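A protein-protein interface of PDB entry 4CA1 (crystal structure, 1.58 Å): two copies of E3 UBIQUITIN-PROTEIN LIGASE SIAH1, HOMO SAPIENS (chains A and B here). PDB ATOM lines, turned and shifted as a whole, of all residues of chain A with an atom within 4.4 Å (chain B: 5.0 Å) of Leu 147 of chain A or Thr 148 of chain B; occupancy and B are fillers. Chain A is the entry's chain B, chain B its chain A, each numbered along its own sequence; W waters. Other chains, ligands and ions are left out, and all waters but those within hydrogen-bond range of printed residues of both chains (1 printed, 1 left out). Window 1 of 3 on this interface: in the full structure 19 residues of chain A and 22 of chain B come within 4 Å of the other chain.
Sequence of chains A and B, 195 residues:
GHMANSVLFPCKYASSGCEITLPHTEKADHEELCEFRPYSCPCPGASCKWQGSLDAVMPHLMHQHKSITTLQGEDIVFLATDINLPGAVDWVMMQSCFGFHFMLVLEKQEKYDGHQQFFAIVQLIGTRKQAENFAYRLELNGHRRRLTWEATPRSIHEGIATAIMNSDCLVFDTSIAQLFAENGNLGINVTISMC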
ATOM      1  N   LEU A 138      18.376  -1.323  30.713  1.00  0.00           N
ATOM      2  CA  LEU A 138      18.745   0.002  31.247  1.00  0.00           C
ATOM      3  C   LEU A 138      17.532   0.882  31.108  1.00  0.00           C
ATOM      4  O   LEU A 138      16.962   0.982  30.011  1.00  0.00           O
ATOM      5  CB  LEU A 138      19.880   0.616  30.426  1.00  0.00           C
ATOM      6  CG  LEU A 138      21.144  -0.286  30.360  1.00  0.00           C
ATOM      7  CD1 LEU A 138      22.227   0.461  29.525  1.00  0.00           C
ATOM      8  CD2 LEU A 138      21.676  -0.586  31.770  1.00  0.00           C
ATOM      9  N   GLU A 139      17.121   1.540  32.192  1.00  0.00           N
ATOM     10  CA  GLU A 139      15.930   2.408  32.064  1.00  0.00           C
ATOM     11  C   GLU A 139      16.316   3.772  32.651  1.00  0.00           C
ATOM     12  O   GLU A 139      16.834   3.895  33.773  1.00  0.00           O
ATOM     13  CB  GLU A 139      14.748   1.764  32.795  1.00  0.00           C
ATOM     14  CG  GLU A 139      13.379   2.341  32.665  1.00  0.00           C
ATOM     15  CD  GLU A 139      12.474   1.400  33.539  1.00  0.00           C
ATOM     16  OE1 GLU A 139      11.903   0.286  33.129  1.00  0.00           O
ATOM     17  OE2 GLU A 139      12.431   1.733  34.703  1.00  0.00           O
ATOM     18  N   LEU A 140      15.994   4.832  31.878  1.00  0.00           N
ATOM     19  CA  LEU A 140      15.982   6.209  32.427  1.00  0.00           C
ATOM     20  C   LEU A 140      14.546   6.599  32.706  1.00  0.00           C
ATOM     21  O   LEU A 140      13.673   6.379  31.859  1.00  0.00           O
ATOM     22  CB  LEU A 140      16.561   7.154  31.337  1.00  0.00           C
ATOM     23  CG  LEU A 140      17.983   6.761  30.814  1.00  0.00           C
ATOM     24  CD1 LEU A 140      18.502   7.869  29.878  1.00  0.00           C
ATOM     25  CD2 LEU A 140      18.966   6.507  31.953  1.00  0.00           C
ATOM     26  N   ARG A 146      10.054   7.797  29.842  1.00  0.00           N
ATOM     27  CA  ARG A 146      10.916   6.624  30.158  1.00  0.00           C
ATOM     28  C   ARG A 146      11.623   6.197  28.902  1.00  0.00           C
ATOM     29  O   ARG A 146      10.967   6.076  27.813  1.00  0.00           O
ATOM     30  CB  ARG A 146      10.016   5.443  30.679  1.00  0.00           C
ATOM     31  CG  ARG A 146      10.927   4.332  31.201  1.00  0.00           C
ATOM     32  CD  ARG A 146      10.183   3.142  31.672  1.00  0.00           C
ATOM     33  NE  ARG A 146       9.455   3.477  32.817  1.00  0.00           N
ATOM     34  CZ  ARG A 146       8.133   3.452  32.882  1.00  0.00           C
ATOM     35  NH1 ARG A 146       7.472   3.159  31.809  1.00  0.00           N
ATOM     36  NH2 ARG A 146       7.508   3.703  34.015  1.00  0.00           N
ATOM     37  N   LEU A 147      12.937   5.968  29.003  1.00  0.00           N
ATOM     38  CA  LEU A 147      13.734   5.503  27.821  1.00  0.00           C
ATOM     39  C   LEU A 147      14.367   4.186  28.269  1.00  0.00           C
ATOM     40  O   LEU A 147      14.975   4.162  29.336  1.00  0.00           O
ATOM     41  CB  LEU A 147      14.817   6.545  27.463  1.00  0.00           C
ATOM     42  CG  LEU A 147      15.709   6.130  26.294  1.00  0.00           C
ATOM     43  CD1 LEU A 147      14.974   5.951  24.962  1.00  0.00           C
ATOM     44  CD2 LEU A 147      16.798   7.240  26.134  1.00  0.00           C
ATOM     45  N   THR A 148      14.173   3.134  27.507  1.00  0.00           N
ATOM     46  CA  THR A 148      14.629   1.780  27.950  1.00  0.00           C
ATOM     47  C   THR A 148      15.425   1.153  26.813  1.00  0.00           C
ATOM     48  O   THR A 148      15.058   1.236  25.641  1.00  0.00           O
ATOM     49  CB  THR A 148      13.381   0.880  28.199  1.00  0.00           C
ATOM     50  OG1 THR A 148      12.505   1.558  29.122  1.00  0.00           O
ATOM     51  CG2 THR A 148      13.912  -0.444  28.847  1.00  0.00           C
ATOM     52  N   LEU A 170      22.533   1.637  24.698  1.00  0.00           N
ATOM     53  CA  LEU A 170      21.672   2.800  24.930  1.00  0.00           C
ATOM     54  C   LEU A 170      22.436   4.085  24.544  1.00  0.00           C
ATOM     55  O   LEU A 170      23.518   4.363  25.116  1.00  0.00           O
ATOM     56  CB  LEU A 170      21.315   2.869  26.399  1.00  0.00           C
ATOM     57  CG  LEU A 170      20.427   4.113  26.741  1.00  0.00           C
ATOM     58  CD1 LEU A 170      19.152   4.207  25.852  1.00  0.00           C
ATOM     59  CD2 LEU A 170      20.074   4.056  28.259  1.00  0.00           C
ATOM     60  N   PHE A 172      22.133   8.307  24.045  1.00  0.00           N
ATOM     61  CA  PHE A 172      21.285   9.507  24.258  1.00  0.00           C
ATOM     62  C   PHE A 172      22.132  10.750  24.343  1.00  0.00           C
ATOM     63  O   PHE A 172      23.144  10.720  24.821  1.00  0.00           O
ATOM     64  CB  PHE A 172      20.342   9.350  25.467  1.00  0.00           C
ATOM     65  CG  PHE A 172      21.047   9.065  26.809  1.00  0.00           C
ATOM     66  CD1 PHE A 172      21.515   7.787  27.114  1.00  0.00           C
ATOM     67  CD2 PHE A 172      21.277  10.077  27.691  1.00  0.00           C
ATOM     68  CE1 PHE A 172      22.109   7.502  28.318  1.00  0.00           C
ATOM     69  CE2 PHE A 172      21.891   9.853  28.921  1.00  0.00           C
ATOM     70  CZ  PHE A 172      22.339   8.550  29.241  1.00  0.00           C
ATOM     71  N   PHE A 180      15.941  13.494  32.308  1.00  0.00           N
ATOM     72  CA  PHE A 180      16.082  12.406  33.267  1.00  0.00           C
ATOM     73  C   PHE A 180      16.958  12.796  34.437  1.00  0.00           C
ATOM     74  O   PHE A 180      16.887  12.160  35.484  1.00  0.00           O
ATOM     75  CB  PHE A 180      16.662  11.214  32.513  1.00  0.00           C
ATOM     76  CG  PHE A 180      15.732  10.737  31.412  1.00  0.00           C
ATOM     77  CD1 PHE A 180      14.492  10.207  31.783  1.00  0.00           C
ATOM     78  CD2 PHE A 180      16.079  10.825  30.055  1.00  0.00           C
ATOM     79  CE1 PHE A 180      13.614   9.720  30.835  1.00  0.00           C
ATOM     80  CE2 PHE A 180      15.160  10.374  29.084  1.00  0.00           C
ATOM     81  CZ  PHE A 180      13.939   9.783  29.465  1.00  0.00           C
ATOM     82  N   ARG B 137       3.871   4.520  23.697  1.00  0.00           N
ATOM     83  CA  ARG B 137       5.112   3.740  23.761  1.00  0.00           C
ATOM     84  C   ARG B 137       5.534   3.437  22.330  1.00  0.00           C
ATOM     85  O   ARG B 137       4.702   2.948  21.539  1.00  0.00           O
ATOM     86  CB  ARG B 137       4.864   2.400  24.495  1.00  0.00           C
ATOM     87  CG  ARG B 137       6.164   1.576  24.503  1.00  0.00           C
ATOM     88  CD  ARG B 137       5.996   0.273  25.279  1.00  0.00           C
ATOM     89  NE  ARG B 137       5.003  -0.547  24.575  1.00  0.00           N
ATOM     90  CZ  ARG B 137       4.413  -1.580  25.177  1.00  0.00           C
ATOM     91  NH1 ARG B 137       4.814  -1.962  26.410  1.00  0.00           N
ATOM     92  NH2 ARG B 137       3.438  -2.278  24.560  1.00  0.00           N
ATOM     93  N   LEU B 138       6.750   3.806  21.948  1.00  0.00           N
ATOM     94  CA  LEU B 138       7.356   3.433  20.690  1.00  0.00           C
ATOM     95  C   LEU B 138       8.412   2.400  20.966  1.00  0.00           C
ATOM     96  O   LEU B 138       9.239   2.616  21.866  1.00  0.00           O
ATOM     97  CB  LEU B 138       8.047   4.639  20.053  1.00  0.00           C
ATOM     98  CG  LEU B 138       7.125   5.856  19.877  1.00  0.00           C
ATOM     99  CD1 LEU B 138       7.901   6.990  19.136  1.00  0.00           C
ATOM    100  CD2 LEU B 138       5.849   5.481  19.047  1.00  0.00           C
ATOM    101  N   GLU B 139       8.360   1.256  20.284  1.00  0.00           N
ATOM    102  CA  GLU B 139       9.382   0.205  20.416  1.00  0.00           C
ATOM    103  C   GLU B 139      10.033  -0.070  19.108  1.00  0.00           C
ATOM    104  O   GLU B 139       9.374  -0.162  18.062  1.00  0.00           O
ATOM    105  CB  GLU B 139       8.776  -1.105  20.876  1.00  0.00           C
ATOM    106  CG  GLU B 139       8.171  -1.081  22.241  1.00  0.00           C
ATOM    107  CD  GLU B 139       7.823  -2.516  22.713  1.00  0.00           C
ATOM    108  OE1 GLU B 139       7.793  -3.479  21.891  1.00  0.00           O
ATOM    109  OE2 GLU B 139       7.576  -2.714  23.918  1.00  0.00           O
ATOM    110  N   ARG B 146      15.992  -4.407  22.164  1.00  0.00           N
ATOM    111  CA  ARG B 146      14.762  -3.607  22.159  1.00  0.00           C
ATOM    112  C   ARG B 146      15.049  -2.226  22.661  1.00  0.00           C
ATOM    113  O   ARG B 146      15.685  -2.047  23.689  1.00  0.00           O
ATOM    114  CB  ARG B 146      13.701  -4.275  23.071  1.00  0.00           C
ATOM    115  CG  ARG B 146      12.364  -3.526  22.985  1.00  0.00           C
ATOM    116  CD  ARG B 146      11.265  -4.114  23.845  1.00  0.00           C
ATOM    117  NE  ARG B 146      10.996  -5.431  23.377  1.00  0.00           N
ATOM    118  CZ  ARG B 146      11.144  -6.505  24.149  1.00  0.00           C
ATOM    119  NH1 ARG B 146      11.606  -6.343  25.357  1.00  0.00           N
ATOM    120  NH2 ARG B 146      10.866  -7.707  23.695  1.00  0.00           N
ATOM    121  N   LEU B 147      14.583  -1.216  21.942  1.00  0.00           N
ATOM    122  CA  LEU B 147      14.729   0.200  22.372  1.00  0.00           C
ATOM    123  C   LEU B 147      13.324   0.729  22.507  1.00  0.00           C
ATOM    124  O   LEU B 147      12.503   0.628  21.551  1.00  0.00           O
ATOM    125  CB  LEU B 147      15.502   0.990  21.301  1.00  0.00           C
ATOM    126  CG  LEU B 147      15.626   2.521  21.569  1.00  0.00           C
ATOM    127  CD1 LEU B 147      16.444   2.777  22.845  1.00  0.00           C
ATOM    128  CD2 LEU B 147      16.358   3.140  20.350  1.00  0.00           C
ATOM    129  N   THR B 148      13.001   1.317  23.668  1.00  0.00           N
ATOM    130  CA  THR B 148      11.620   1.784  23.936  1.00  0.00           C
ATOM    131  C   THR B 148      11.605   3.200  24.428  1.00  0.00           C
ATOM    132  O   THR B 148      12.457   3.606  25.272  1.00  0.00           O
ATOM    133  CB  THR B 148      10.993   0.908  25.077  1.00  0.00           C
ATOM    134  OG1 THR B 148      11.105  -0.501  24.740  1.00  0.00           O
ATOM    135  CG2 THR B 148       9.506   1.247  25.253  1.00  0.00           C
ATOM    136  N   TRP B 149      10.677   4.026  23.930  1.00  0.00           N
ATOM    137  CA  TRP B 149      10.449   5.400  24.428  1.00  0.00           C
ATOM    138  C   TRP B 149       9.041   5.509  24.864  1.00  0.00           C
ATOM    139  O   TRP B 149       8.134   5.057  24.112  1.00  0.00           O
ATOM    140  CB  TRP B 149      10.725   6.329  23.292  1.00  0.00           C
ATOM    141  CG  TRP B 149      10.230   7.716  23.507  1.00  0.00           C
ATOM    142  CD1 TRP B 149       9.094   8.294  22.934  1.00  0.00           C
ATOM    143  CD2 TRP B 149      10.778   8.734  24.403  1.00  0.00           C
ATOM    144  NE1 TRP B 149       8.939   9.612  23.332  1.00  0.00           N
ATOM    145  CE2 TRP B 149       9.951   9.914  24.237  1.00  0.00           C
ATOM    146  CE3 TRP B 149      11.921   8.778  25.263  1.00  0.00           C
ATOM    147  CZ2 TRP B 149      10.204  11.118  24.903  1.00  0.00           C
ATOM    148  CZ3 TRP B 149      12.129  10.025  25.907  1.00  0.00           C
ATOM    149  CH2 TRP B 149      11.279  11.138  25.735  1.00  0.00           C
ATOM    150  N   GLU B 150       8.766   6.110  26.000  1.00  0.00           N
ATOM    151  CA  GLU B 150       7.379   6.308  26.446  1.00  0.00           C
ATOM    152  C   GLU B 150       7.239   7.702  26.907  1.00  0.00           C
ATOM    153  O   GLU B 150       8.098   8.246  27.647  1.00  0.00           O
ATOM    154  CB  GLU B 150       7.068   5.353  27.610  1.00  0.00           C
ATOM    155  CG  GLU B 150       7.137   3.886  27.154  1.00  0.00           C
ATOM    156  CD  GLU B 150       7.023   2.977  28.323  1.00  0.00           C
ATOM    157  OE1 GLU B 150       5.879   2.607  28.722  1.00  0.00           O
ATOM    158  OE2 GLU B 150       8.113   2.644  28.902  1.00  0.00           O
ATOM    159  N   LEU B 170      11.644   9.911  20.822  1.00  0.00           N
ATOM    160  CA  LEU B 170      12.611   8.827  20.516  1.00  0.00           C
ATOM    161  C   LEU B 170      13.577   9.335  19.476  1.00  0.00           C
ATOM    162  O   LEU B 170      13.183   9.845  18.416  1.00  0.00           O
ATOM    163  CB  LEU B 170      11.776   7.639  19.968  1.00  0.00           C
ATOM    164  CG  LEU B 170      12.682   6.488  19.439  1.00  0.00           C
ATOM    165  CD1 LEU B 170      13.553   5.889  20.564  1.00  0.00           C
ATOM    166  CD2 LEU B 170      11.831   5.338  18.894  1.00  0.00           C
HETATM  167  O   HOH W   1      13.459  -1.638  25.682  1.00  0.00           O
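Water W1 lies within hydrogen-bond range of the side-chain hydroxyl of Thr 148 of chain B (2.8 Å), the backbone carbonyl oxygen of Arg 146 of chain B (3.0 Å) and the backbone carbonyl oxygen of Thr 148 of chain A (3.3 Å).
Arg 146 of chain A touches Thr 148 of chain B, and with the chains exchanged Thr 148 of chain A touches Arg 146 of chain B.
Leu 147 of chain A touches Thr 148 of chain B, and with the chains exchanged Thr 148 of chain A touches Leu 147 of chain B.
Thr 148 of chain A touches its own counterpart, Thr 148 of chain B.
Leu 147 of chain A touches one residue of chain B.
Of the printed residues of chain A, Thr 148 of chain B touches Arg 146 (3.8 Å), Leu 147 (3.4 Å) and Thr 148 (2.9 Å).
Of the printed residues of chain A, Arg 146 of chain B touches Thr 148 (3.9 Å).
Of the printed residues of chain B, Phe 180 of chain A touches Trp 149 (3.999 Å).
Of the printed residues of chain A, Leu 147 of chain B touches Thr 148 (3.4 Å).
Of the printed residues of chain A, Glu 150 of chain B touches Arg 146 (2.9 Å).
Glu 139 of chain A touches none of the printed residues of chain B.
The nearest residue of chain B that does not touch Leu 147 of chain A is Leu 147 of chain B (4.1 Å).
Hydrophobic or aromatic side chains of chain A that line the printed part of chain B: Leu 147 and Phe 180.
Among the printed residues, 8 pairs touch across the chains.
Among the printed residues, Asp or Glu carboxylates within 4 Å of a Lys or Arg side-chain nitrogen of the other chain: Arg 146 of chain A with Glu 150 of chain B (3.0 Å).
The guanidinium group (NH1) of Arg 146 of chain A lies within salt-bridge range of the side-chain carboxylate (OE2) of Glu 150 of chain B (3.0 Å).
The backbone carbonyl oxygen (O) of Thr 148 of chain A lies within hydrogen-bond range of the backbone NH (N) of Thr 148 of chain B, 2.9 Å away.
The backbone NH (N) of Leu 138 of chain B sits at hydrogen-bond distance from the backbone carbonyl oxygen (O) of Trp 149 of chain B (2.9 Å).
The side-chain carboxylate of Glu 139 of chain A lies within salt-bridge range of the guanidinium group of Arg 146 of chain A, 3.9 Å away.
O of Leu 147 of chain A lies within hydrogen-bond range of N of Leu 140 of chain A, 2.8 Å away.
Among the printed residues, pairs that only touch across the chains: Arg 146 of chain A with Thr 148 of chain B (3.8 Å), Arg 146 of chain A with Trp 149 of chain B (3.5 Å), Leu 147 of chain A with Thr 148 of chain B (3.4 Å), Thr 148 of chain A with Arg 146 of chain B (3.9 Å), Thr 148 of chain A with Leu 147 of chain B (3.4 Å) and Phe 180 of chain A with Trp 149 of chain B (3.999 Å).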
